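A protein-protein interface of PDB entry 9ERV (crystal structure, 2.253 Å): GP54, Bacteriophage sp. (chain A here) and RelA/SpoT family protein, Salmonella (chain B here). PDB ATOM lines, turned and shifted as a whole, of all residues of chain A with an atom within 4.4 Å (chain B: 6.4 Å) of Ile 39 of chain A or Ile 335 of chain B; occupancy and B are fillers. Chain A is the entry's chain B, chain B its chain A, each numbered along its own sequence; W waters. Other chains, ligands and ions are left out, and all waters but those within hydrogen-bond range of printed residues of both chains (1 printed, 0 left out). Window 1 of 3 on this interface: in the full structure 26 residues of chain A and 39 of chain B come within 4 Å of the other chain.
OG of Ser 261 of chain B is in hydrogen-bond range of O of Ile 39 of chain A (3.4 Å).
OG1 of Thr 262 of chain B sits at hydrogen-bond distance from O of Ile 37 of chain A, at 3.3 Å.
The backbone carbonyl oxygen (O) of Asp 327 of chain B lies within hydrogen-bond range of the side-chain amino group (NZ) of Lys 35 of chain A (2.9 Å).
The backbone carbonyl oxygen (O) of Val 333 of chain B lies within hydrogen-bond range of the side-chain amino group (NZ) of Lys 35 of chain A (3.3 Å).
O of Leu 334 of chain B sits at hydrogen-bond distance from N of Gly 36 of chain A (3.4 Å).
O of Ala 336 of chain B lies within hydrogen-bond range of N of Lys 35 of chain A.
The side-chain hydroxyl (OG1) of Thr 262 of chain B lies within hydrogen-bond range of the backbone carbonyl oxygen (O) of Ser 258 of chain B (2.8 Å).
The side-chain carboxylate (OD2) of Asp 327 of chain B is in salt-bridge range of the guanidinium group (NH1) of Arg 290 of chain B (2.8 Å).
N of Leu 334 of chain B sits at hydrogen-bond distance from O of Met 291 of chain B (2.9 Å).
O of Ile 335 of chain B sits at hydrogen-bond distance from N of Met 291 of chain B (3.0 Å).
The backbone carbonyl oxygen (O) of Thr 40 of chain A is in hydrogen-bond range of the side-chain sulfur (SG) of Cys 48 of chain A.
N of Tyr 49 of chain A is in hydrogen-bond range of O of Thr 40 of chain A, at 2.9 Å.
Among the printed residues, pairs that only touch across the chains: Gly 36 of chain A with Thr 262 of chain B (3.2 Å), Ile 39 of chain A with Met 291 of chain B (3.4 Å), Lys 35 of chain A with Leu 334 of chain B (3.5 Å), Lys 35 of chain A with Ile 335 of chain B (3.5 Å), Ile 37 of chain A with Ser 261 of chain B (3.5 Å), Glu 38 of chain A with Arg 257 of chain B (3.7 Å), Ile 39 of chain A with Phe 265 of chain B (3.7 Å), Ile 37 of chain A with Ser 258 of chain B (3.7 Å), Glu 38 of chain A with Ser 261 of chain B (3.7 Å), Thr 40 of chain A with Asn 359 of chain B (3.8 Å), Gly 36 of chain A with Ser 258 of chain B (3.8 Å), His 50 of chain A with Met 291 of chain B (3.9 Å), Ile 37 of chain A with Ile 335 of chain B (3.9 Å), Glu 38 of chain A with Ser 258 of chain B (3.97 Å), Lys 35 of chain A with Thr 262 of chain B (3.98 Å) and Ile 39 of chain A with Ile 335 of chain B (3.997 Å).
Printed residues of chain B within 4 Å of Ile 39 of chain A: Ser 261, Phe 265, Met 291 and Ile 335.
Tyr 49 of chain A touches none of the printed residues of chain B.
Of the printed residues of chain B, His 50 of chain A touches Met 291 (3.9 Å).
Of the printed residues of chain A, Arg 257 of chain B touches Glu 38 (3.7 Å).
Val 289 of chain B touches none of the printed residues of chain A.
Printed residues of chain A within 4 Å of Val 333 of chain B: Lys 35 (3.3 Å).
Printed residues of chain A within 4 Å of Ile 335 of chain B: Lys 35, Ile 37 and Ile 39.
Of the printed residues of chain A, Ala 336 of chain B touches Lys 35 (3.0 Å).
The nearest printed residue of chain B that does not touch Ile 39 of chain A is Thr 262 of chain B (4.6 Å).
Printed residues of chain A that touch a printed residue of chain B: Lys 35, Gly 36, Ile 37, Glu 38, Ile 39, Thr 40 and His 50.
Hydrophobic or aromatic side chains of chain A that line the printed part of chain B: Ile 37, Ile 39 and His 50.
Among the printed residues, 22 pairs touch across the chains.
Among the printed residues, no Asp or Glu carboxylate lies within 4 Å of a Lys or Arg side-chain nitrogen of the other chain.
Water W1 lies within hydrogen-bond range of the backbone carbonyl oxygen (O) of Ile 39 of chain A and the backbone carbonyl oxygen (O) of Ser 261 of chain B.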
ATOM      1  N   LYS A  35     -14.786 -14.606  12.829  1.00  0.00           N
ATOM      2  CA  LYS A  35     -14.734 -14.964  14.243  1.00  0.00           C
ATOM      3  C   LYS A  35     -15.281 -13.842  15.113  1.00  0.00           C
ATOM      4  O   LYS A  35     -15.128 -12.667  14.787  1.00  0.00           O
ATOM      5  CB  LYS A  35     -13.274 -15.187  14.676  1.00  0.00           C
ATOM      6  CG  LYS A  35     -12.687 -16.520  14.317  1.00  0.00           C
ATOM      7  CD  LYS A  35     -11.189 -16.415  14.411  1.00  0.00           C
ATOM      8  CE  LYS A  35     -10.530 -17.753  14.449  1.00  0.00           C
ATOM      9  NZ  LYS A  35      -9.094 -17.628  14.138  1.00  0.00           N
ATOM     10  N   GLY A  36     -15.808 -14.210  16.264  1.00  0.00           N
ATOM     11  CA  GLY A  36     -16.309 -13.247  17.216  1.00  0.00           C
ATOM     12  C   GLY A  36     -16.709 -13.883  18.517  1.00  0.00           C
ATOM     13  O   GLY A  36     -16.866 -15.100  18.604  1.00  0.00           O
ATOM     14  N   ILE A  37     -16.845 -13.065  19.541  1.00  0.00           N
ATOM     15  CA  ILE A  37     -17.247 -13.488  20.888  1.00  0.00           C
ATOM     16  C   ILE A  37     -18.225 -12.426  21.462  1.00  0.00           C
ATOM     17  O   ILE A  37     -18.453 -11.385  20.834  1.00  0.00           O
ATOM     18  CB  ILE A  37     -15.987 -13.643  21.816  1.00  0.00           C
ATOM     19  CG1 ILE A  37     -15.224 -12.308  21.952  1.00  0.00           C
ATOM     20  CG2 ILE A  37     -15.067 -14.801  21.406  1.00  0.00           C
ATOM     21  CD1 ILE A  37     -14.227 -12.291  23.038  1.00  0.00           C
ATOM     22  N   GLU A  38     -18.804 -12.684  22.643  1.00  0.00           N
ATOM     23  CA  GLU A  38     -19.629 -11.679  23.300  1.00  0.00           C
ATOM     24  C   GLU A  38     -18.636 -10.743  23.983  1.00  0.00           C
ATOM     25  O   GLU A  38     -17.799 -11.187  24.767  1.00  0.00           O
ATOM     26  CB  GLU A  38     -20.673 -12.302  24.247  1.00  0.00           C
ATOM     27  CG  GLU A  38     -21.867 -12.808  23.464  1.00  0.00           C
ATOM     28  CD  GLU A  38     -22.867 -13.643  24.234  1.00  0.00           C
ATOM     29  OE1 GLU A  38     -23.811 -13.060  24.818  1.00  0.00           O
ATOM     30  OE2 GLU A  38     -22.729 -14.888  24.226  1.00  0.00           O
ATOM     31  N   ILE A  39     -18.628  -9.485  23.556  1.00  0.00           N
ATOM     32  CA  ILE A  39     -17.715  -8.464  24.039  1.00  0.00           C
ATOM     33  C   ILE A  39     -18.377  -7.089  24.028  1.00  0.00           C
ATOM     34  O   ILE A  39     -19.193  -6.796  23.155  1.00  0.00           O
ATOM     35  CB  ILE A  39     -16.438  -8.473  23.146  1.00  0.00           C
ATOM     36  CG1 ILE A  39     -15.420  -7.440  23.610  1.00  0.00           C
ATOM     37  CG2 ILE A  39     -16.755  -8.310  21.646  1.00  0.00           C
ATOM     38  CD1 ILE A  39     -14.133  -7.765  23.178  1.00  0.00           C
ATOM     39  N   THR A  40     -18.062  -6.261  25.018  1.00  0.00           N
ATOM     40  CA  THR A  40     -18.498  -4.872  25.057  1.00  0.00           C
ATOM     41  C   THR A  40     -17.296  -3.997  25.358  1.00  0.00           C
ATOM     42  O   THR A  40     -16.427  -4.391  26.127  1.00  0.00           O
ATOM     43  CB  THR A  40     -19.652  -4.576  26.041  1.00  0.00           C
ATOM     44  OG1 THR A  40     -19.217  -4.765  27.385  1.00  0.00           O
ATOM     45  CG2 THR A  40     -20.936  -5.341  25.740  1.00  0.00           C
ATOM     46  N   CYS A  48     -13.214  -2.852  28.983  1.00  0.00           N
ATOM     47  CA  CYS A  48     -13.726  -3.865  28.069  1.00  0.00           C
ATOM     48  C   CYS A  48     -14.175  -5.083  28.846  1.00  0.00           C
ATOM     49  O   CYS A  48     -13.603  -5.401  29.875  1.00  0.00           O
ATOM     50  CB  CYS A  48     -12.685  -4.231  27.017  1.00  0.00           C
ATOM     51  SG  CYS A  48     -13.322  -5.283  25.695  1.00  0.00           S
ATOM     52  N   TYR A  49     -15.198  -5.767  28.357  1.00  0.00           N
ATOM     53  CA  TYR A  49     -15.747  -6.937  29.020  1.00  0.00           C
ATOM     54  C   TYR A  49     -15.814  -8.115  28.073  1.00  0.00           C
ATOM     55  O   TYR A  49     -16.554  -8.072  27.096  1.00  0.00           O
ATOM     56  CB  TYR A  49     -17.159  -6.639  29.545  1.00  0.00           C
ATOM     57  CG  TYR A  49     -17.206  -5.565  30.606  1.00  0.00           C
ATOM     58  CD1 TYR A  49     -16.842  -5.838  31.918  1.00  0.00           C
ATOM     59  CD2 TYR A  49     -17.635  -4.280  30.303  1.00  0.00           C
ATOM     60  CE1 TYR A  49     -16.916  -4.863  32.906  1.00  0.00           C
ATOM     61  CE2 TYR A  49     -17.697  -3.291  31.279  1.00  0.00           C
ATOM     62  CZ  TYR A  49     -17.338  -3.588  32.582  1.00  0.00           C
ATOM     63  OH  TYR A  49     -17.385  -2.612  33.553  1.00  0.00           O
ATOM     64  N   HIS A  50     -15.076  -9.177  28.381  1.00  0.00           N
ATOM     65  CA  HIS A  50     -15.108 -10.417  27.618  1.00  0.00           C
ATOM     66  C   HIS A  50     -14.578 -11.585  28.435  1.00  0.00           C
ATOM     67  O   HIS A  50     -13.772 -11.389  29.345  1.00  0.00           O
ATOM     68  CB  HIS A  50     -14.418 -10.313  26.238  1.00  0.00           C
ATOM     69  CG  HIS A  50     -12.923 -10.209  26.276  1.00  0.00           C
ATOM     70  ND1 HIS A  50     -12.121 -11.334  26.356  1.00  0.00           N
ATOM     71  CD2 HIS A  50     -12.132  -9.114  26.189  1.00  0.00           C
ATOM     72  CE1 HIS A  50     -10.878 -10.888  26.338  1.00  0.00           C
ATOM     73  NE2 HIS A  50     -10.834  -9.558  26.254  1.00  0.00           N
ATOM     74  N   ARG B 257     -25.908 -13.832  19.194  1.00  0.00           N
ATOM     75  CA  ARG B 257     -25.315 -13.007  20.252  1.00  0.00           C
ATOM     76  C   ARG B 257     -23.845 -12.583  19.956  1.00  0.00           C
ATOM     77  O   ARG B 257     -23.513 -11.425  20.178  1.00  0.00           O
ATOM     78  CB  ARG B 257     -25.469 -13.655  21.611  1.00  0.00           C
ATOM     79  CG  ARG B 257     -26.882 -13.453  22.165  1.00  0.00           C
ATOM     80  CD  ARG B 257     -27.123 -14.322  23.378  1.00  0.00           C
ATOM     81  NE  ARG B 257     -26.782 -15.727  23.130  1.00  0.00           N
ATOM     82  CZ  ARG B 257     -26.787 -16.675  24.059  1.00  0.00           C
ATOM     83  NH1 ARG B 257     -27.126 -16.384  25.314  1.00  0.00           N
ATOM     84  NH2 ARG B 257     -26.465 -17.920  23.744  1.00  0.00           N
ATOM     85  N   SER B 258     -23.018 -13.487  19.372  1.00  0.00           N
ATOM     86  CA  SER B 258     -21.629 -13.232  18.983  1.00  0.00           C
ATOM     87  C   SER B 258     -21.529 -12.286  17.816  1.00  0.00           C
ATOM     88  O   SER B 258     -20.774 -11.313  17.900  1.00  0.00           O
ATOM     89  CB  SER B 258     -20.898 -14.528  18.667  1.00  0.00           C
ATOM     90  OG  SER B 258     -20.484 -15.027  19.917  1.00  0.00           O
ATOM     91  N   SER B 261     -22.648  -8.785  19.037  1.00  0.00           N
ATOM     92  CA  SER B 261     -21.639  -8.177  19.913  1.00  0.00           C
ATOM     93  C   SER B 261     -20.408  -7.697  19.134  1.00  0.00           C
ATOM     94  O   SER B 261     -19.948  -6.577  19.355  1.00  0.00           O
ATOM     95  CB  SER B 261     -21.193  -9.173  20.986  1.00  0.00           C
ATOM     96  OG  SER B 261     -21.732  -8.789  22.237  1.00  0.00           O
ATOM     97  N   THR B 262     -19.868  -8.555  18.251  1.00  0.00           N
ATOM     98  CA  THR B 262     -18.688  -8.273  17.444  1.00  0.00           C
ATOM     99  C   THR B 262     -18.905  -7.080  16.535  1.00  0.00           C
ATOM    100  O   THR B 262     -18.073  -6.184  16.538  1.00  0.00           O
ATOM    101  CB  THR B 262     -18.268  -9.532  16.691  1.00  0.00           C
ATOM    102  OG1 THR B 262     -18.044 -10.549  17.651  1.00  0.00           O
ATOM    103  CG2 THR B 262     -17.015  -9.332  15.860  1.00  0.00           C
ATOM    104  N   THR B 264     -21.077  -4.610  16.891  1.00  0.00           N
ATOM    105  CA  THR B 264     -21.211  -3.428  17.721  1.00  0.00           C
ATOM    106  C   THR B 264     -19.852  -2.957  18.230  1.00  0.00           C
ATOM    107  O   THR B 264     -19.585  -1.758  18.230  1.00  0.00           O
ATOM    108  CB  THR B 264     -22.208  -3.721  18.850  1.00  0.00           C
ATOM    109  OG1 THR B 264     -23.469  -4.036  18.253  1.00  0.00           O
ATOM    110  CG2 THR B 264     -22.361  -2.537  19.834  1.00  0.00           C
ATOM    111  N   PHE B 265     -19.002  -3.900  18.667  1.00  0.00           N
ATOM    112  CA  PHE B 265     -17.641  -3.667  19.153  1.00  0.00           C
ATOM    113  C   PHE B 265     -16.776  -3.043  18.045  1.00  0.00           C
ATOM    114  O   PHE B 265     -16.083  -2.063  18.296  1.00  0.00           O
ATOM    115  CB  PHE B 265     -17.040  -5.010  19.637  1.00  0.00           C
ATOM    116  CG  PHE B 265     -15.554  -5.067  19.874  1.00  0.00           C
ATOM    117  CD1 PHE B 265     -15.007  -4.593  21.050  1.00  0.00           C
ATOM    118  CD2 PHE B 265     -14.717  -5.692  18.969  1.00  0.00           C
ATOM    119  CE1 PHE B 265     -13.637  -4.662  21.274  1.00  0.00           C
ATOM    120  CE2 PHE B 265     -13.352  -5.758  19.195  1.00  0.00           C
ATOM    121  CZ  PHE B 265     -12.820  -5.249  20.347  1.00  0.00           C
ATOM    122  N   VAL B 289     -11.154  -5.609  11.763  1.00  0.00           N
ATOM    123  CA  VAL B 289     -11.055  -5.598  13.218  1.00  0.00           C
ATOM    124  C   VAL B 289     -10.656  -6.986  13.684  1.00  0.00           C
ATOM    125  O   VAL B 289     -11.315  -7.954  13.340  1.00  0.00           O
ATOM    126  CB  VAL B 289     -12.365  -5.100  13.864  1.00  0.00           C
ATOM    127  CG1 VAL B 289     -12.212  -4.974  15.375  1.00  0.00           C
ATOM    128  CG2 VAL B 289     -12.791  -3.768  13.250  1.00  0.00           C
ATOM    129  N   ARG B 290      -9.549  -7.086  14.424  1.00  0.00           N
ATOM    130  CA  ARG B 290      -8.990  -8.349  14.876  1.00  0.00           C
ATOM    131  C   ARG B 290      -8.600  -8.270  16.356  1.00  0.00           C
ATOM    132  O   ARG B 290      -8.037  -7.265  16.784  1.00  0.00           O
ATOM    133  CB  ARG B 290      -7.751  -8.698  14.010  1.00  0.00           C
ATOM    134  CG  ARG B 290      -6.722  -9.641  14.671  1.00  0.00           C
ATOM    135  CD  ARG B 290      -5.532 -10.020  13.797  1.00  0.00           C
ATOM    136  NE  ARG B 290      -4.508  -8.975  13.704  1.00  0.00           N
ATOM    137  CZ  ARG B 290      -4.293  -8.226  12.623  1.00  0.00           C
ATOM    138  NH1 ARG B 290      -5.033  -8.394  11.532  1.00  0.00           N
ATOM    139  NH2 ARG B 290      -3.340  -7.302  12.627  1.00  0.00           N
ATOM    140  N   MET B 291      -8.885  -9.326  17.133  1.00  0.00           N
ATOM    141  CA  MET B 291      -8.428  -9.390  18.518  1.00  0.00           C
ATOM    142  C   MET B 291      -7.634 -10.672  18.694  1.00  0.00           C
ATOM    143  O   MET B 291      -8.091 -11.738  18.280  1.00  0.00           O
ATOM    144  CB  MET B 291      -9.544  -9.307  19.574  1.00  0.00           C
ATOM    145  CG  MET B 291      -8.969  -9.241  20.984  1.00  0.00           C
ATOM    146  SD  MET B 291     -10.096  -9.623  22.340  1.00  0.00           S
ATOM    147  CE  MET B 291     -10.780  -8.140  22.590  1.00  0.00           C
ATOM    148  N   ARG B 292      -6.435 -10.563  19.255  1.00  0.00           N
ATOM    149  CA  ARG B 292      -5.613 -11.740  19.478  1.00  0.00           C
ATOM    150  C   ARG B 292      -4.974 -11.779  20.853  1.00  0.00           C
ATOM    151  O   ARG B 292      -4.841 -10.752  21.510  1.00  0.00           O
ATOM    152  CB  ARG B 292      -4.549 -11.868  18.388  1.00  0.00           C
ATOM    153  CG  ARG B 292      -3.498 -10.765  18.427  1.00  0.00           C
ATOM    154  CD  ARG B 292      -2.122 -11.283  18.038  1.00  0.00           C
ATOM    155  NE  ARG B 292      -2.179 -12.109  16.833  1.00  0.00           N
ATOM    156  CZ  ARG B 292      -2.162 -11.636  15.593  1.00  0.00           C
ATOM    157  NH1 ARG B 292      -2.023 -10.333  15.375  1.00  0.00           N
ATOM    158  NH2 ARG B 292      -2.270 -12.462  14.559  1.00  0.00           N
ATOM    159  N   VAL B 307      -5.966  -5.564  20.271  1.00  0.00           N
ATOM    160  CA  VAL B 307      -7.063  -5.270  19.368  1.00  0.00           C
ATOM    161  C   VAL B 307      -6.550  -4.288  18.329  1.00  0.00           C
ATOM    162  O   VAL B 307      -6.005  -3.260  18.702  1.00  0.00           O
ATOM    163  CB  VAL B 307      -8.256  -4.649  20.137  1.00  0.00           C
ATOM    164  CG1 VAL B 307      -9.395  -4.252  19.190  1.00  0.00           C
ATOM    165  CG2 VAL B 307      -8.734  -5.576  21.236  1.00  0.00           C
ATOM    166  N   ASP B 327      -6.132 -14.458   9.492  1.00  0.00           N
ATOM    167  CA  ASP B 327      -6.548 -14.272  10.883  1.00  0.00           C
ATOM    168  C   ASP B 327      -7.605 -15.309  11.296  1.00  0.00           C
ATOM    169  O   ASP B 327      -7.629 -15.731  12.453  1.00  0.00           O
ATOM    170  CB  ASP B 327      -7.038 -12.836  11.126  1.00  0.00           C
ATOM    171  CG  ASP B 327      -5.977 -11.784  10.841  1.00  0.00           C
ATOM    172  OD1 ASP B 327      -4.762 -12.115  10.934  1.00  0.00           O
ATOM    173  OD2 ASP B 327      -6.355 -10.631  10.520  1.00  0.00           O
ATOM    174  N   VAL B 333      -6.255 -15.766  17.384  1.00  0.00           N
ATOM    175  CA  VAL B 333      -7.243 -14.754  17.040  1.00  0.00           C
ATOM    176  C   VAL B 333      -8.659 -15.184  17.498  1.00  0.00           C
ATOM    177  O   VAL B 333      -9.116 -16.272  17.157  1.00  0.00           O
ATOM    178  CB  VAL B 333      -7.179 -14.482  15.522  1.00  0.00           C
ATOM    179  CG1 VAL B 333      -8.338 -13.611  15.072  1.00  0.00           C
ATOM    180  CG2 VAL B 333      -5.836 -13.858  15.136  1.00  0.00           C
ATOM    181  N   LEU B 334      -9.337 -14.326  18.280  1.00  0.00           N
ATOM    182  CA  LEU B 334     -10.676 -14.568  18.830  1.00  0.00           C
ATOM    183  C   LEU B 334     -11.774 -13.824  18.056  1.00  0.00           C
ATOM    184  O   LEU B 334     -12.927 -14.257  18.050  1.00  0.00           O
ATOM    185  CB  LEU B 334     -10.736 -14.133  20.306  1.00  0.00           C
ATOM    186  CG  LEU B 334      -9.749 -14.788  21.237  1.00  0.00           C
ATOM    187  CD1 LEU B 334      -8.499 -13.984  21.308  1.00  0.00           C
ATOM    188  CD2 LEU B 334     -10.313 -14.878  22.635  1.00  0.00           C
ATOM    189  N   ILE B 335     -11.423 -12.666  17.476  1.00  0.00           N
ATOM    190  CA  ILE B 335     -12.299 -11.803  16.692  1.00  0.00           C
ATOM    191  C   ILE B 335     -11.606 -11.531  15.361  1.00  0.00           C
ATOM    192  O   ILE B 335     -10.450 -11.164  15.352  1.00  0.00           O
ATOM    193  CB  ILE B 335     -12.562 -10.467  17.462  1.00  0.00           C
ATOM    194  CG1 ILE B 335     -13.460 -10.712  18.687  1.00  0.00           C
ATOM    195  CG2 ILE B 335     -13.172  -9.418  16.545  1.00  0.00           C
ATOM    196  CD1 ILE B 335     -13.549  -9.588  19.630  1.00  0.00           C
ATOM    197  N   ALA B 336     -12.310 -11.681  14.257  1.00  0.00           N
ATOM    198  CA  ALA B 336     -11.808 -11.398  12.917  1.00  0.00           C
ATOM    199  C   ALA B 336     -13.029 -11.030  12.098  1.00  0.00           C
ATOM    200  O   ALA B 336     -13.895 -11.873  11.897  1.00  0.00           O
ATOM    201  CB  ALA B 336     -11.129 -12.626  12.333  1.00  0.00           C
ATOM    202  N   VAL B 337     -13.168  -9.752  11.733  1.00  0.00           N
ATOM    203  CA  VAL B 337     -14.325  -9.277  10.978  1.00  0.00           C
ATOM    204  C   VAL B 337     -13.886  -8.188   9.987  1.00  0.00           C
ATOM    205  O   VAL B 337     -12.987  -7.398  10.294  1.00  0.00           O
ATOM    206  CB  VAL B 337     -15.509  -8.823  11.910  1.00  0.00           C
ATOM    207  CG1 VAL B 337     -15.085  -7.744  12.901  1.00  0.00           C
ATOM    208  CG2 VAL B 337     -16.727  -8.364  11.109  1.00  0.00           C
ATOM    209  N   ASN B 359     -27.051  -4.114  22.954  1.00  0.00           N
ATOM    210  CA  ASN B 359     -26.806  -4.631  24.305  1.00  0.00           C
ATOM    211  C   ASN B 359     -28.119  -5.144  24.907  1.00  0.00           C
ATOM    212  O   ASN B 359     -28.173  -6.275  25.412  1.00  0.00           O
ATOM    213  CB  ASN B 359     -26.227  -3.548  25.235  1.00  0.00           C
ATOM    214  CG  ASN B 359     -24.785  -3.181  24.981  1.00  0.00           C
ATOM    215  OD1 ASN B 359     -24.059  -3.845  24.217  1.00  0.00           O
ATOM    216  ND2 ASN B 359     -24.340  -2.084  25.611  1.00  0.00           N
HETATM  217  O   HOH W   1     -20.382  -5.094  21.723  1.00  0.00           O
